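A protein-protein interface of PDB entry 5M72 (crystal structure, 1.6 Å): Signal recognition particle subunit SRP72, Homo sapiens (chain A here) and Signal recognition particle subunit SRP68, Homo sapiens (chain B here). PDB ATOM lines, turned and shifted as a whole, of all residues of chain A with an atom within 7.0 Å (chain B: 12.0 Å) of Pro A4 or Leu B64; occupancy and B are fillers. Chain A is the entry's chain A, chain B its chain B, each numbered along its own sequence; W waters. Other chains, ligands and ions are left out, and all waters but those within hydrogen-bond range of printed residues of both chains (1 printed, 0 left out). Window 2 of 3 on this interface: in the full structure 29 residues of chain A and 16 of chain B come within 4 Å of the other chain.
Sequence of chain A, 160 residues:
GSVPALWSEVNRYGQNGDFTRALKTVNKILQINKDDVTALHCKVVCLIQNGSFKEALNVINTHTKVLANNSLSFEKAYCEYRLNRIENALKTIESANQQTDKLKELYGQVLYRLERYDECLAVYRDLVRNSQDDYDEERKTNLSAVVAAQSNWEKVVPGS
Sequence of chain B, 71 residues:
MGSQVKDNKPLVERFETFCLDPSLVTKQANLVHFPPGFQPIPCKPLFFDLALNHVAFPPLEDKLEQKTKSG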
ATOM      1  N   SER A   2     -17.880  -5.486  17.212  1.00  0.00           N
ATOM      2  CA  SER A   2     -18.502  -6.800  17.098  1.00  0.00           C
ATOM      3  C   SER A   2     -18.459  -7.295  15.663  1.00  0.00           C
ATOM      4  O   SER A   2     -19.036  -6.683  14.760  1.00  0.00           O
ATOM      5  CB  SER A   2     -19.948  -6.765  17.581  1.00  0.00           C
ATOM      6  OG  SER A   2     -20.661  -7.902  17.125  1.00  0.00           O
ATOM      7  N   VAL A   3     -17.783  -8.414  15.444  1.00  0.00           N
ATOM      8  CA  VAL A   3     -17.702  -8.921  14.081  1.00  0.00           C
ATOM      9  C   VAL A   3     -19.004  -9.619  13.686  1.00  0.00           C
ATOM     10  O   VAL A   3     -19.356  -9.552  12.506  1.00  0.00           O
ATOM     11  CB  VAL A   3     -16.458  -9.802  13.870  1.00  0.00           C
ATOM     12  CG1 VAL A   3     -15.200  -8.960  14.053  1.00  0.00           C
ATOM     13  CG2 VAL A   3     -16.433 -10.992  14.802  1.00  0.00           C
ATOM     14  N   PRO A   4     -19.788 -10.242  14.588  1.00  0.00           N
ATOM     15  CA  PRO A   4     -21.136 -10.645  14.150  1.00  0.00           C
ATOM     16  C   PRO A   4     -21.966  -9.474  13.656  1.00  0.00           C
ATOM     17  O   PRO A   4     -22.697  -9.614  12.670  1.00  0.00           O
ATOM     18  CB  PRO A   4     -21.735 -11.297  15.404  1.00  0.00           C
ATOM     19  CG  PRO A   4     -20.557 -11.821  16.125  1.00  0.00           C
ATOM     20  CD  PRO A   4     -19.514 -10.761  15.945  1.00  0.00           C
ATOM     21  N   ALA A   5     -21.858  -8.307  14.297  1.00  0.00           N
ATOM     22  CA  ALA A   5     -22.589  -7.140  13.814  1.00  0.00           C
ATOM     23  C   ALA A   5     -22.122  -6.729  12.422  1.00  0.00           C
ATOM     24  O   ALA A   5     -22.940  -6.351  11.576  1.00  0.00           O
ATOM     25  CB  ALA A   5     -22.443  -5.977  14.799  1.00  0.00           C
ATOM     26  N   LEU A   6     -20.810  -6.784  12.163  1.00  0.00           N
ATOM     27  CA  LEU A   6     -20.313  -6.479  10.822  1.00  0.00           C
ATOM     28  C   LEU A   6     -20.862  -7.460   9.797  1.00  0.00           C
ATOM     29  O   LEU A   6     -21.235  -7.068   8.686  1.00  0.00           O
ATOM     30  CB  LEU A   6     -18.786  -6.499  10.801  1.00  0.00           C
ATOM     31  CG  LEU A   6     -18.096  -5.398  11.608  1.00  0.00           C
ATOM     32  CD1 LEU A   6     -16.595  -5.629  11.646  1.00  0.00           C
ATOM     33  CD2 LEU A   6     -18.413  -4.022  11.026  1.00  0.00           C
ATOM     34  N   TRP A   7     -20.907  -8.745  10.147  1.00  0.00           N
ATOM     35  CA  TRP A   7     -21.440  -9.727   9.214  1.00  0.00           C
ATOM     36  C   TRP A   7     -22.923  -9.496   8.953  1.00  0.00           C
ATOM     37  O   TRP A   7     -23.391  -9.675   7.822  1.00  0.00           O
ATOM     38  CB  TRP A   7     -21.180 -11.139   9.740  1.00  0.00           C
ATOM     39  CG  TRP A   7     -19.809 -11.611   9.396  1.00  0.00           C
ATOM     40  CD1 TRP A   7     -18.774 -11.844  10.254  1.00  0.00           C
ATOM     41  CD2 TRP A   7     -19.319 -11.895   8.081  1.00  0.00           C
ATOM     42  NE1 TRP A   7     -17.666 -12.269   9.547  1.00  0.00           N
ATOM     43  CE2 TRP A   7     -17.977 -12.304   8.213  1.00  0.00           C
ATOM     44  CE3 TRP A   7     -19.887 -11.843   6.804  1.00  0.00           C
ATOM     45  CZ2 TRP A   7     -17.193 -12.659   7.114  1.00  0.00           C
ATOM     46  CZ3 TRP A   7     -19.106 -12.195   5.717  1.00  0.00           C
ATOM     47  CH2 TRP A   7     -17.776 -12.605   5.882  1.00  0.00           C
ATOM     48  N   SER A   8     -23.680  -9.093   9.982  1.00  0.00           N
ATOM     49  CA  SER A   8     -25.075  -8.728   9.764  1.00  0.00           C
ATOM     50  C   SER A   8     -25.182  -7.593   8.750  1.00  0.00           C
ATOM     51  O   SER A   8     -26.068  -7.603   7.882  1.00  0.00           O
ATOM     52  CB  SER A   8     -25.735  -8.343  11.095  1.00  0.00           C
ATOM     53  OG  SER A   8     -27.099  -8.059  10.897  1.00  0.00           O
ATOM     54  N   GLU A   9     -24.259  -6.628   8.829  1.00  0.00           N
ATOM     55  CA  GLU A   9     -24.217  -5.532   7.865  1.00  0.00           C
ATOM     56  C   GLU A   9     -23.910  -6.046   6.462  1.00  0.00           C
ATOM     57  O   GLU A   9     -24.572  -5.668   5.485  1.00  0.00           O
ATOM     58  CB  GLU A   9     -23.169  -4.514   8.321  1.00  0.00           C
ATOM     59  CG  GLU A   9     -23.304  -3.136   7.736  1.00  0.00           C
ATOM     60  CD  GLU A   9     -22.403  -2.135   8.433  1.00  0.00           C
ATOM     61  OE1 GLU A   9     -22.614  -1.888   9.639  1.00  0.00           O
ATOM     62  OE2 GLU A   9     -21.476  -1.607   7.785  1.00  0.00           O
ATOM     63  N   VAL A  10     -22.892  -6.902   6.335  1.00  0.00           N
ATOM     64  CA  VAL A  10     -22.542  -7.452   5.021  1.00  0.00           C
ATOM     65  C   VAL A  10     -23.750  -8.148   4.407  1.00  0.00           C
ATOM     66  O   VAL A  10     -24.043  -8.004   3.207  1.00  0.00           O
ATOM     67  CB  VAL A  10     -21.347  -8.420   5.130  1.00  0.00           C
ATOM     68  CG1 VAL A  10     -21.134  -9.166   3.793  1.00  0.00           C
ATOM     69  CG2 VAL A  10     -20.078  -7.682   5.518  1.00  0.00           C
ATOM     70  N   ASN A  11     -24.441  -8.953   5.212  1.00  0.00           N
ATOM     71  CA  ASN A  11     -25.588  -9.699   4.702  1.00  0.00           C
ATOM     72  C   ASN A  11     -26.698  -8.763   4.248  1.00  0.00           C
ATOM     73  O   ASN A  11     -27.299  -8.967   3.184  1.00  0.00           O
ATOM     74  CB  ASN A  11     -26.104 -10.665   5.766  1.00  0.00           C
ATOM     75  CG  ASN A  11     -27.308 -11.453   5.293  1.00  0.00           C
ATOM     76  OD1 ASN A  11     -27.214 -12.259   4.354  1.00  0.00           O
ATOM     77  ND2 ASN A  11     -28.453 -11.225   5.934  1.00  0.00           N
ATOM     78  N   PHE B  57     -22.855 -14.052  -2.727  1.00  0.00           N
ATOM     79  CA  PHE B  57     -22.235 -14.395  -1.457  1.00  0.00           C
ATOM     80  C   PHE B  57     -22.537 -15.847  -1.090  1.00  0.00           C
ATOM     81  O   PHE B  57     -23.627 -16.357  -1.376  1.00  0.00           O
ATOM     82  CB  PHE B  57     -22.755 -13.502  -0.328  1.00  0.00           C
ATOM     83  CG  PHE B  57     -22.316 -12.068  -0.404  1.00  0.00           C
ATOM     84  CD1 PHE B  57     -21.335 -11.651  -1.295  1.00  0.00           C
ATOM     85  CD2 PHE B  57     -22.884 -11.127   0.459  1.00  0.00           C
ATOM     86  CE1 PHE B  57     -20.951 -10.326  -1.339  1.00  0.00           C
ATOM     87  CE2 PHE B  57     -22.507  -9.813   0.415  1.00  0.00           C
ATOM     88  CZ  PHE B  57     -21.533  -9.403  -0.479  1.00  0.00           C
ATOM     89  N   PRO B  58     -21.611 -16.519  -0.416  1.00  0.00           N
ATOM     90  CA  PRO B  58     -21.932 -17.799   0.221  1.00  0.00           C
ATOM     91  C   PRO B  58     -22.884 -17.588   1.386  1.00  0.00           C
ATOM     92  O   PRO B  58     -23.111 -16.443   1.804  1.00  0.00           O
ATOM     93  CB  PRO B  58     -20.562 -18.301   0.702  1.00  0.00           C
ATOM     94  CG  PRO B  58     -19.779 -17.044   0.940  1.00  0.00           C
ATOM     95  CD  PRO B  58     -20.224 -16.092  -0.147  1.00  0.00           C
ATOM     96  N   PRO B  59     -23.472 -18.657   1.922  1.00  0.00           N
ATOM     97  CA  PRO B  59     -24.354 -18.513   3.092  1.00  0.00           C
ATOM     98  C   PRO B  59     -23.602 -17.908   4.269  1.00  0.00           C
ATOM     99  O   PRO B  59     -22.485 -18.321   4.586  1.00  0.00           O
ATOM    100  CB  PRO B  59     -24.792 -19.953   3.380  1.00  0.00           C
ATOM    101  CG  PRO B  59     -24.659 -20.656   2.060  1.00  0.00           C
ATOM    102  CD  PRO B  59     -23.478 -20.030   1.383  1.00  0.00           C
ATOM    103  N   LEU B  60     -24.234 -16.932   4.932  1.00  0.00           N
ATOM    104  CA  LEU B  60     -23.572 -16.146   5.967  1.00  0.00           C
ATOM    105  C   LEU B  60     -24.110 -16.395   7.367  1.00  0.00           C
ATOM    106  O   LEU B  60     -23.646 -15.743   8.307  1.00  0.00           O
ATOM    107  CB  LEU B  60     -23.681 -14.647   5.650  1.00  0.00           C
ATOM    108  CG  LEU B  60     -23.058 -14.159   4.340  1.00  0.00           C
ATOM    109  CD1 LEU B  60     -23.177 -12.646   4.229  1.00  0.00           C
ATOM    110  CD2 LEU B  60     -21.604 -14.603   4.227  1.00  0.00           C
ATOM    111  N   GLU B  61     -25.066 -17.317   7.535  1.00  0.00           N
ATOM    112  CA  GLU B  61     -25.670 -17.533   8.851  1.00  0.00           C
ATOM    113  C   GLU B  61     -24.628 -17.849   9.912  1.00  0.00           C
ATOM    114  O   GLU B  61     -24.732 -17.373  11.051  1.00  0.00           O
ATOM    115  CB  GLU B  61     -26.685 -18.671   8.800  1.00  0.00           C
ATOM    116  CG  GLU B  61     -28.041 -18.292   8.270  1.00  0.00           C
ATOM    117  CD  GLU B  61     -28.188 -18.604   6.805  1.00  0.00           C
ATOM    118  OE1 GLU B  61     -27.150 -18.699   6.109  1.00  0.00           O
ATOM    119  OE2 GLU B  61     -29.342 -18.760   6.354  1.00  0.00           O
ATOM    120  N   ASP B  62     -23.641 -18.684   9.573  1.00  0.00           N
ATOM    121  CA  ASP B  62     -22.660 -19.121  10.559  1.00  0.00           C
ATOM    122  C   ASP B  62     -21.761 -17.989  11.008  1.00  0.00           C
ATOM    123  O   ASP B  62     -21.200 -18.056  12.105  1.00  0.00           O
ATOM    124  CB  ASP B  62     -21.797 -20.248  10.000  1.00  0.00           C
ATOM    125  CG  ASP B  62     -22.579 -21.520   9.775  1.00  0.00           C
ATOM    126  OD1 ASP B  62     -23.674 -21.656  10.361  1.00  0.00           O
ATOM    127  OD2 ASP B  62     -22.097 -22.387   9.016  1.00  0.00           O
ATOM    128  N   LYS B  63     -21.605 -16.957  10.185  1.00  0.00           N
ATOM    129  CA  LYS B  63     -20.780 -15.831  10.584  1.00  0.00           C
ATOM    130  C   LYS B  63     -21.460 -14.975  11.641  1.00  0.00           C
ATOM    131  O   LYS B  63     -20.826 -14.072  12.190  1.00  0.00           O
ATOM    132  CB  LYS B  63     -20.426 -14.994   9.357  1.00  0.00           C
ATOM    133  CG  LYS B  63     -19.977 -15.824   8.157  1.00  0.00           C
ATOM    134  CD  LYS B  63     -18.762 -16.700   8.486  1.00  0.00           C
ATOM    135  CE  LYS B  63     -17.506 -15.861   8.710  1.00  0.00           C
ATOM    136  NZ  LYS B  63     -16.315 -16.704   9.035  1.00  0.00           N
ATOM    137  N   LEU B  64     -22.727 -15.238  11.938  1.00  0.00           N
ATOM    138  CA  LEU B  64     -23.408 -14.540  13.013  1.00  0.00           C
ATOM    139  C   LEU B  64     -23.069 -15.208  14.340  1.00  0.00           C
ATOM    140  O   LEU B  64     -23.317 -14.646  15.408  1.00  0.00           O
ATOM    141  CB  LEU B  64     -24.921 -14.525  12.785  1.00  0.00           C
ATOM    142  CG  LEU B  64     -25.538 -13.356  12.005  1.00  0.00           C
ATOM    143  CD1 LEU B  64     -24.792 -13.048  10.726  1.00  0.00           C
ATOM    144  CD2 LEU B  64     -27.009 -13.630  11.712  1.00  0.00           C
HETATM  145  O   HOH W   1     -26.700 -15.529   3.806  1.00  0.00           O
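Of the 8 printed residues of chain B, 4 touch a printed residue of chain A. Printed residues of chain B that touch a printed residue of chain A: Phe B57, Leu B60, Lys B63 and Leu B64. Of the 10 printed residues of chain A, 4 touch a printed residue of chain B. Printed residues of chain A that touch a printed residue of chain B: Pro A4, Trp A7, Val A10 and Asn A11. Hydrophobic or aromatic side chains of chain A that line the printed part of chain B: Pro A4, Trp A7 and Val A10. Among the printed residues, 6 pairs touch across the chains.
Water W1 bridges N of Leu B60 (3.1 Å) and OD1 of Asn A11 (3.4 Å).
No residue of chain B comes within 4 Å of Val A3. Of chain B, only Lys B63 and Leu B64 come within 4 Å of Pro A4. Of the printed residues of chain B, Trp A7 touches Leu B60 and Lys B63. No residue of chain B comes within 4 Å of Ser A8. Of the printed residues of chain B, Asn A11 touches Leu B60 (3.8 Å). Of the printed residues of chain A, Phe B57 touches Val A10. Printed residues of chain A within 4 Å of Leu B60: Trp A7 and Asn A11. Printed residues of chain A within 4 Å of Lys B63: Pro A4 (3.96 Å) and Trp A7 (3.4 Å). Of chain A, only Pro A4 (3.7 Å) comes within 4 Å of Leu B64. The nearest residue of chain B that does not touch Pro A4 is Asp B62 (7.4 Å).
Lys B63 touches Pro A4 (O to CA, 3.96 Å). Pro A4 touches Leu B64. Trp A7 touches Leu B60. Trp A7 touches Lys B63 (CG to CB, 3.4 Å). Val A10 touches Phe B57. CA of Asn A11 touches CD1 of Leu B60, at 3.8 Å.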
